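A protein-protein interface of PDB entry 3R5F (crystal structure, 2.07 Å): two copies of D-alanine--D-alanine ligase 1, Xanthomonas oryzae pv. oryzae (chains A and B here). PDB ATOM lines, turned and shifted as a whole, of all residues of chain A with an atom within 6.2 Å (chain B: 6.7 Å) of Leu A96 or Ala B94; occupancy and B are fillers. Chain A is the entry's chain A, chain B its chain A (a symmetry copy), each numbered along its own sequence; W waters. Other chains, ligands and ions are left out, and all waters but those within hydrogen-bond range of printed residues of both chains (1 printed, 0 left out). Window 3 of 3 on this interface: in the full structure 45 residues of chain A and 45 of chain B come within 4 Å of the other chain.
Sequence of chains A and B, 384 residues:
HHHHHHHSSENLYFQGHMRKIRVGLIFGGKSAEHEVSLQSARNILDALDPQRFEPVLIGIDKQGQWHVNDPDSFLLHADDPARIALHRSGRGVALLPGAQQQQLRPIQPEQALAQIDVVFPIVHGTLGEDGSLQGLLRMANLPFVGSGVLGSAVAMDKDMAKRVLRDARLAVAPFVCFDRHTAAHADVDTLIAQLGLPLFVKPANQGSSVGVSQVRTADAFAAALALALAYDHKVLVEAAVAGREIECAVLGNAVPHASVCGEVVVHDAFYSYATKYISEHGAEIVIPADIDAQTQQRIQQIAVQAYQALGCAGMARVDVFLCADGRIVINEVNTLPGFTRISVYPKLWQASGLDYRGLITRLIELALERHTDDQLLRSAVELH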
ATOM      1  N   ALA A  94      18.989  11.863   2.161  1.00  0.00           N
ATOM      2  CA  ALA A  94      17.943  11.516   3.062  1.00  0.00           C
ATOM      3  C   ALA A  94      16.870  10.847   2.275  1.00  0.00           C
ATOM      4  O   ALA A  94      16.633  11.156   1.146  1.00  0.00           O
ATOM      5  CB  ALA A  94      17.395  12.725   3.734  1.00  0.00           C
ATOM      6  N   LEU A  95      16.240   9.903   2.907  1.00  0.00           N
ATOM      7  CA  LEU A  95      15.180   9.159   2.332  1.00  0.00           C
ATOM      8  C   LEU A  95      13.929   9.406   3.148  1.00  0.00           C
ATOM      9  O   LEU A  95      13.949   9.354   4.350  1.00  0.00           O
ATOM     10  CB  LEU A  95      15.570   7.720   2.375  1.00  0.00           C
ATOM     11  CG  LEU A  95      14.575   6.635   2.088  1.00  0.00           C
ATOM     12  CD1 LEU A  95      15.250   5.433   2.537  1.00  0.00           C
ATOM     13  CD2 LEU A  95      13.306   6.759   2.805  1.00  0.00           C
ATOM     14  N   LEU A  96      12.842   9.726   2.503  1.00  0.00           N
ATOM     15  CA  LEU A  96      11.688   9.920   3.281  1.00  0.00           C
ATOM     16  C   LEU A  96      10.810   8.732   3.057  1.00  0.00           C
ATOM     17  O   LEU A  96      10.156   8.645   2.058  1.00  0.00           O
ATOM     18  CB  LEU A  96      11.003  11.156   2.781  1.00  0.00           C
ATOM     19  CG  LEU A  96      11.901  12.356   2.550  1.00  0.00           C
ATOM     20  CD1 LEU A  96      11.107  13.550   2.451  1.00  0.00           C
ATOM     21  CD2 LEU A  96      12.880  12.547   3.596  1.00  0.00           C
ATOM     22  N   PRO A  97      10.702   7.895   4.074  1.00  0.00           N
ATOM     23  CA  PRO A  97       9.964   6.642   3.978  1.00  0.00           C
ATOM     24  C   PRO A  97       8.567   6.999   3.737  1.00  0.00           C
ATOM     25  O   PRO A  97       8.128   7.917   4.345  1.00  0.00           O
ATOM     26  CB  PRO A  97      10.077   6.061   5.369  1.00  0.00           C
ATOM     27  CG  PRO A  97      11.156   6.753   6.014  1.00  0.00           C
ATOM     28  CD  PRO A  97      11.467   7.994   5.312  1.00  0.00           C
ATOM     29  N   GLY A  98       7.885   6.295   2.857  1.00  0.00           N
ATOM     30  CA  GLY A  98       6.481   6.612   2.634  1.00  0.00           C
ATOM     31  C   GLY A  98       6.247   7.870   1.811  1.00  0.00           C
ATOM     32  O   GLY A  98       5.122   8.199   1.508  1.00  0.00           O
ATOM     33  N   ALA A  99       7.310   8.567   1.428  1.00  0.00           N
ATOM     34  CA  ALA A  99       7.171   9.681   0.484  1.00  0.00           C
ATOM     35  C   ALA A  99       6.837   9.131  -0.892  1.00  0.00           C
ATOM     36  O   ALA A  99       7.224   7.991  -1.262  1.00  0.00           O
ATOM     37  CB  ALA A  99       8.454  10.514   0.416  1.00  0.00           C
ATOM     38  N   GLN A 100       6.133   9.952  -1.648  1.00  0.00           N
ATOM     39  CA  GLN A 100       5.634   9.535  -2.937  1.00  0.00           C
ATOM     40  C   GLN A 100       6.316  10.340  -4.069  1.00  0.00           C
ATOM     41  O   GLN A 100       6.198   9.974  -5.218  1.00  0.00           O
ATOM     42  CB  GLN A 100       4.094   9.647  -2.989  1.00  0.00           C
ATOM     43  CG  GLN A 100       3.373   8.517  -3.800  1.00  0.00           C
ATOM     44  CD  GLN A 100       3.104   7.235  -2.995  1.00  0.00           C
ATOM     45  OE1 GLN A 100       2.592   7.278  -1.866  1.00  0.00           O
ATOM     46  NE2 GLN A 100       3.414   6.089  -3.595  1.00  0.00           N
ATOM     47  N   GLN A 101       7.063  11.385  -3.697  1.00  0.00           N
ATOM     48  CA  GLN A 101       7.747  12.278  -4.616  1.00  0.00           C
ATOM     49  C   GLN A 101       8.968  12.834  -3.913  1.00  0.00           C
ATOM     50  O   GLN A 101       8.923  13.002  -2.701  1.00  0.00           O
ATOM     51  CB  GLN A 101       6.736  13.383  -4.918  1.00  0.00           C
ATOM     52  CG  GLN A 101       7.189  14.684  -5.428  1.00  0.00           C
ATOM     53  CD  GLN A 101       6.094  15.282  -6.334  1.00  0.00           C
ATOM     54  OE1 GLN A 101       4.892  15.006  -6.149  1.00  0.00           O
ATOM     55  NE2 GLN A 101       6.507  16.044  -7.328  1.00  0.00           N
ATOM     56  N   GLN A 102      10.043  13.142  -4.632  1.00  0.00           N
ATOM     57  CA  GLN A 102      11.287  13.591  -3.973  1.00  0.00           C
ATOM     58  C   GLN A 102      11.616  12.705  -2.739  1.00  0.00           C
ATOM     59  O   GLN A 102      11.905  13.205  -1.664  1.00  0.00           O
ATOM     60  CB  GLN A 102      11.215  15.079  -3.516  1.00  0.00           C
ATOM     61  CG  GLN A 102      11.434  16.116  -4.613  1.00  0.00           C
ATOM     62  CD  GLN A 102      12.872  16.157  -5.065  1.00  0.00           C
ATOM     63  OE1 GLN A 102      13.161  16.021  -6.245  1.00  0.00           O
ATOM     64  NE2 GLN A 102      13.789  16.319  -4.127  1.00  0.00           N
ATOM     65  N   GLN A 103      11.559  11.398  -2.921  1.00  0.00           N
ATOM     66  CA  GLN A 103      11.807  10.463  -1.816  1.00  0.00           C
ATOM     67  C   GLN A 103      13.231  10.505  -1.328  1.00  0.00           C
ATOM     68  O   GLN A 103      13.500  10.274  -0.132  1.00  0.00           O
ATOM     69  CB  GLN A 103      11.465   9.068  -2.235  1.00  0.00           C
ATOM     70  CG  GLN A 103      10.128   8.955  -2.745  1.00  0.00           C
ATOM     71  CD  GLN A 103      10.116   9.082  -4.243  1.00  0.00           C
ATOM     72  OE1 GLN A 103      10.671  10.051  -4.828  1.00  0.00           O
ATOM     73  NE2 GLN A 103       9.474   8.129  -4.881  1.00  0.00           N
ATOM     74  N   LEU A 104      14.140  10.803  -2.271  1.00  0.00           N
ATOM     75  CA  LEU A 104      15.561  10.977  -1.991  1.00  0.00           C
ATOM     76  C   LEU A 104      15.942  12.418  -1.966  1.00  0.00           C
ATOM     77  O   LEU A 104      15.767  13.145  -2.939  1.00  0.00           O
ATOM     78  CB  LEU A 104      16.419  10.191  -2.968  1.00  0.00           C
ATOM     79  CG  LEU A 104      16.771   8.770  -2.504  1.00  0.00           C
ATOM     80  CD1 LEU A 104      15.567   7.954  -2.129  1.00  0.00           C
ATOM     81  CD2 LEU A 104      17.476   8.060  -3.586  1.00  0.00           C
ATOM     82  N   ARG A 105      16.375  12.869  -0.813  1.00  0.00           N
ATOM     83  CA  ARG A 105      16.592  14.272  -0.571  1.00  0.00           C
ATOM     84  C   ARG A 105      17.928  14.671  -0.058  1.00  0.00           C
ATOM     85  O   ARG A 105      18.556  13.992   0.696  1.00  0.00           O
ATOM     86  CB  ARG A 105      15.549  14.822   0.374  1.00  0.00           C
ATOM     87  CG  ARG A 105      14.428  15.418  -0.380  1.00  0.00           C
ATOM     88  CD  ARG A 105      13.293  15.794   0.476  1.00  0.00           C
ATOM     89  NE  ARG A 105      12.068  15.357  -0.122  1.00  0.00           N
ATOM     90  CZ  ARG A 105      10.885  15.807   0.208  1.00  0.00           C
ATOM     91  NH1 ARG A 105      10.771  16.721   1.133  1.00  0.00           N
ATOM     92  NH2 ARG A 105       9.820  15.338  -0.389  1.00  0.00           N
ATOM     93  N   MET A 139      10.400   0.936   0.496  1.00  0.00           N
ATOM     94  CA  MET A 139       9.801   1.803   1.555  1.00  0.00           C
ATOM     95  C   MET A 139       9.763   3.258   1.051  1.00  0.00           C
ATOM     96  O   MET A 139       8.952   4.068   1.521  1.00  0.00           O
ATOM     97  CB  MET A 139      10.619   1.778   2.824  1.00  0.00           C
ATOM     98  CG  MET A 139      10.547   0.446   3.561  1.00  0.00           C
ATOM     99  SD  MET A 139       8.852   0.010   4.052  1.00  0.00           S
ATOM    100  CE  MET A 139       8.284   1.417   5.068  1.00  0.00           C
ATOM    101  N   ALA A 140      10.593   3.542   0.039  1.00  0.00           N
ATOM    102  CA  ALA A 140      10.579   4.848  -0.558  1.00  0.00           C
ATOM    103  C   ALA A 140       9.690   4.864  -1.801  1.00  0.00           C
ATOM    104  O   ALA A 140       9.604   5.854  -2.450  1.00  0.00           O
ATOM    105  CB  ALA A 140      12.024   5.302  -0.901  1.00  0.00           C
ATOM    106  N   TRP B  66       4.500   8.856   7.573  1.00  0.00           N
ATOM    107  CA  TRP B  66       5.100   8.729   8.897  1.00  0.00           C
ATOM    108  C   TRP B  66       4.919  10.014   9.721  1.00  0.00           C
ATOM    109  O   TRP B  66       5.038  11.100   9.177  1.00  0.00           O
ATOM    110  CB  TRP B  66       6.606   8.398   8.742  1.00  0.00           C
ATOM    111  CG  TRP B  66       6.926   6.997   8.194  1.00  0.00           C
ATOM    112  CD1 TRP B  66       6.217   6.292   7.248  1.00  0.00           C
ATOM    113  CD2 TRP B  66       8.046   6.164   8.566  1.00  0.00           C
ATOM    114  NE1 TRP B  66       6.834   5.078   7.026  1.00  0.00           N
ATOM    115  CE2 TRP B  66       7.946   4.978   7.833  1.00  0.00           C
ATOM    116  CE3 TRP B  66       9.144   6.330   9.460  1.00  0.00           C
ATOM    117  CZ2 TRP B  66       8.908   3.916   7.947  1.00  0.00           C
ATOM    118  CZ3 TRP B  66      10.062   5.306   9.599  1.00  0.00           C
ATOM    119  CH2 TRP B  66       9.944   4.098   8.836  1.00  0.00           C
ATOM    120  N   GLY B  92       6.989  14.905  10.132  1.00  0.00           N
ATOM    121  CA  GLY B  92       7.555  13.920   9.225  1.00  0.00           C
ATOM    122  C   GLY B  92       8.887  13.378   9.690  1.00  0.00           C
ATOM    123  O   GLY B  92       9.511  13.920  10.625  1.00  0.00           O
ATOM    124  N   VAL B  93       9.326  12.307   9.029  1.00  0.00           N
ATOM    125  CA  VAL B  93      10.519  11.550   9.419  1.00  0.00           C
ATOM    126  C   VAL B  93      11.451  11.386   8.208  1.00  0.00           C
ATOM    127  O   VAL B  93      10.987  11.086   7.132  1.00  0.00           O
ATOM    128  CB  VAL B  93      10.145  10.084   9.947  1.00  0.00           C
ATOM    129  CG1 VAL B  93      11.335   9.380  10.448  1.00  0.00           C
ATOM    130  CG2 VAL B  93       9.106  10.103  11.055  1.00  0.00           C
ATOM    131  N   ALA B  94      12.736  11.470   8.453  1.00  0.00           N
ATOM    132  CA  ALA B  94      13.733  11.227   7.466  1.00  0.00           C
ATOM    133  C   ALA B  94      14.667  10.204   8.011  1.00  0.00           C
ATOM    134  O   ALA B  94      14.925  10.143   9.176  1.00  0.00           O
ATOM    135  CB  ALA B  94      14.481  12.473   7.147  1.00  0.00           C
ATOM    136  N   LEU B  95      15.154   9.386   7.127  1.00  0.00           N
ATOM    137  CA  LEU B  95      16.070   8.353   7.446  1.00  0.00           C
ATOM    138  C   LEU B  95      17.363   8.616   6.704  1.00  0.00           C
ATOM    139  O   LEU B  95      17.362   8.906   5.535  1.00  0.00           O
ATOM    140  CB  LEU B  95      15.458   7.064   7.013  1.00  0.00           C
ATOM    141  CG  LEU B  95      16.261   5.799   6.961  1.00  0.00           C
ATOM    142  CD1 LEU B  95      15.415   4.893   6.212  1.00  0.00           C
ATOM    143  CD2 LEU B  95      17.550   5.915   6.280  1.00  0.00           C
ATOM    144  N   LEU B  96      18.472   8.567   7.388  1.00  0.00           N
ATOM    145  CA  LEU B  96      19.659   8.785   6.669  1.00  0.00           C
ATOM    146  C   LEU B  96      20.333   7.459   6.532  1.00  0.00           C
ATOM    147  O   LEU B  96      20.941   6.993   7.451  1.00  0.00           O
ATOM    148  CB  LEU B  96      20.520   9.708   7.478  1.00  0.00           C
ATOM    149  CG  LEU B  96      19.818  10.922   8.055  1.00  0.00           C
ATOM    150  CD1 LEU B  96      20.789  11.898   8.466  1.00  0.00           C
ATOM    151  CD2 LEU B  96      18.906  11.550   7.127  1.00  0.00           C
ATOM    152  N   GLN B 102      21.614   9.365  15.127  1.00  0.00           N
ATOM    153  CA  GLN B 102      20.473  10.172  14.649  1.00  0.00           C
ATOM    154  C   GLN B 102      20.035   9.730  13.224  1.00  0.00           C
ATOM    155  O   GLN B 102      19.854  10.549  12.339  1.00  0.00           O
ATOM    156  CB  GLN B 102      20.789  11.698  14.623  1.00  0.00           C
ATOM    157  CG  GLN B 102      20.713  12.408  15.970  1.00  0.00           C
ATOM    158  CD  GLN B 102      19.289  12.548  16.449  1.00  0.00           C
ATOM    159  OE1 GLN B 102      18.956  12.136  17.551  1.00  0.00           O
ATOM    160  NE2 GLN B 102      18.431  13.109  15.615  1.00  0.00           N
ATOM    161  N   GLN B 103      19.880   8.432  13.033  1.00  0.00           N
ATOM    162  CA  GLN B 103      19.512   7.895  11.716  1.00  0.00           C
ATOM    163  C   GLN B 103      18.124   8.297  11.292  1.00  0.00           C
ATOM    164  O   GLN B 103      17.850   8.454  10.085  1.00  0.00           O
ATOM    165  CB  GLN B 103      19.618   6.402  11.720  1.00  0.00           C
ATOM    166  CG  GLN B 103      20.909   5.941  12.149  1.00  0.00           C
ATOM    167  CD  GLN B 103      20.906   5.641  13.621  1.00  0.00           C
ATOM    168  OE1 GLN B 103      20.498   6.483  14.466  1.00  0.00           O
ATOM    169  NE2 GLN B 103      21.375   4.458  13.954  1.00  0.00           N
ATOM    170  N   LEU B 104      17.252   8.459  12.301  1.00  0.00           N
ATOM    171  CA  LEU B 104      15.884   8.928  12.113  1.00  0.00           C
ATOM    172  C   LEU B 104      15.737  10.360  12.499  1.00  0.00           C
ATOM    173  O   LEU B 104      16.003  10.749  13.633  1.00  0.00           O
ATOM    174  CB  LEU B 104      14.890   8.046  12.851  1.00  0.00           C
ATOM    175  CG  LEU B 104      14.327   6.886  12.016  1.00  0.00           C
ATOM    176  CD1 LEU B 104      15.395   6.027  11.401  1.00  0.00           C
ATOM    177  CD2 LEU B 104      13.495   6.024  12.873  1.00  0.00           C
ATOM    178  N   ARG B 105      15.407  11.178  11.528  1.00  0.00           N
ATOM    179  CA  ARG B 105      15.420  12.608  11.693  1.00  0.00           C
ATOM    180  C   ARG B 105      14.177  13.341  11.342  1.00  0.00           C
ATOM    181  O   ARG B 105      13.467  13.008  10.443  1.00  0.00           O
ATOM    182  CB  ARG B 105      16.559  13.227  10.916  1.00  0.00           C
ATOM    183  CG  ARG B 105      17.742  13.404  11.781  1.00  0.00           C
ATOM    184  CD  ARG B 105      18.942  13.819  11.038  1.00  0.00           C
ATOM    185  NE  ARG B 105      20.068  13.044  11.463  1.00  0.00           N
ATOM    186  CZ  ARG B 105      21.316  13.375  11.245  1.00  0.00           C
ATOM    187  NH1 ARG B 105      21.593  14.481  10.608  1.00  0.00           N
ATOM    188  NH2 ARG B 105      22.278  12.595  11.662  1.00  0.00           N
ATOM    189  N   PRO B 106      13.902  14.355  12.117  1.00  0.00           N
ATOM    190  CA  PRO B 106      12.743  15.171  11.853  1.00  0.00           C
ATOM    191  C   PRO B 106      12.951  16.027  10.653  1.00  0.00           C
ATOM    192  O   PRO B 106      13.983  16.620  10.466  1.00  0.00           O
ATOM    193  CB  PRO B 106      12.634  16.033  13.096  1.00  0.00           C
ATOM    194  CG  PRO B 106      13.893  15.952  13.730  1.00  0.00           C
ATOM    195  CD  PRO B 106      14.495  14.657  13.415  1.00  0.00           C
ATOM    196  N   ILE B 107      11.909  16.145   9.873  1.00  0.00           N
ATOM    197  CA  ILE B 107      11.905  17.002   8.735  1.00  0.00           C
ATOM    198  C   ILE B 107      11.683  18.472   9.111  1.00  0.00           C
ATOM    199  O   ILE B 107      11.932  19.344   8.330  1.00  0.00           O
ATOM    200  CB  ILE B 107      10.849  16.533   7.752  1.00  0.00           C
ATOM    201  CG1 ILE B 107      10.973  15.029   7.579  1.00  0.00           C
ATOM    202  CG2 ILE B 107      11.049  17.180   6.440  1.00  0.00           C
ATOM    203  CD1 ILE B 107      10.251  14.473   6.437  1.00  0.00           C
ATOM    204  N   LEU B 113      14.699  14.928  17.272  1.00  0.00           N
ATOM    205  CA  LEU B 113      14.111  13.651  17.690  1.00  0.00           C
ATOM    206  C   LEU B 113      15.173  12.881  18.492  1.00  0.00           C
ATOM    207  O   LEU B 113      16.351  12.827  18.094  1.00  0.00           O
ATOM    208  CB  LEU B 113      13.660  12.849  16.450  1.00  0.00           C
ATOM    209  CG  LEU B 113      13.034  11.472  16.667  1.00  0.00           C
ATOM    210  CD1 LEU B 113      11.554  11.635  16.849  1.00  0.00           C
ATOM    211  CD2 LEU B 113      13.329  10.507  15.534  1.00  0.00           C
HETATM  212  O   HOH W   1       6.261   9.551   5.095  1.00  0.00           O
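Among the printed residues, pairs that only touch across the chains: Ala A94 with Leu B95, Ala A94 with Leu B96, Leu A95 with Ala B94, Leu A96 with Ala B94, Pro A97 with Trp B66, Pro A97 with Val B93 and Met A139 with Trp B66.
Of the printed residues of chain A, Val B93 touches Pro A97 (3.6 Å). Printed residues of chain B within 4 Å of Pro A97: Trp B66 and Val B93. Of the printed residues of chain B, Met A139 touches Trp B66 (3.9 Å). Printed residues of chain B within 4 Å of Leu A95: Ala B94 (3.6 Å) and Leu B95 (3.0 Å). Gln A103 touches none of the printed residues of chain B. The nearest residue of chain B that does not touch Leu A96 is Val B93 (4.1 Å). The nearest printed residue of chain A that does not touch Ala B94 is Ala A94 (4.5 Å). The nearest printed residue of chain A that does not touch Val B93 is Leu A96 (4.1 Å).
N of Leu A96 sits at hydrogen-bond distance from O of Gln A103, at 2.8 Å. O of Ala B94 is in hydrogen-bond range of N of Arg B105. N of Leu B96 is in hydrogen-bond range of O of Gln B103. O of Ala A94 is in hydrogen-bond range of N of Arg A105, at 2.6 Å. The backbone NH (N) of Gly A98 lies within hydrogen-bond range of the backbone carbonyl oxygen (O) of Met A139 (2.8 Å).
Ala A94 touches Leu B95, and with the chains exchanged Leu A95 touches Ala B94. Ala A94 touches Leu B96, and with the chains exchanged Leu A96 touches Ala B94. Leu B95 touches its own counterpart, Leu A95. Positions printed for both chains: 94, 95, 96, 102, 103, 104 and 105. Of the 8 pairs that touch across the chains among the printed residues, 5 have their exchanged pair printed and touching as well.
Water W1 bridges O of Pro A97 (2.6 Å) and N of Trp B66 (3.1 Å).
The backbone NH of Leu A95 lies within hydrogen-bond range of the backbone carbonyl oxygen of Leu B95 (3.0 Å).
Of the 13 printed residues of chain B, 5 touch a printed residue of chain A.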
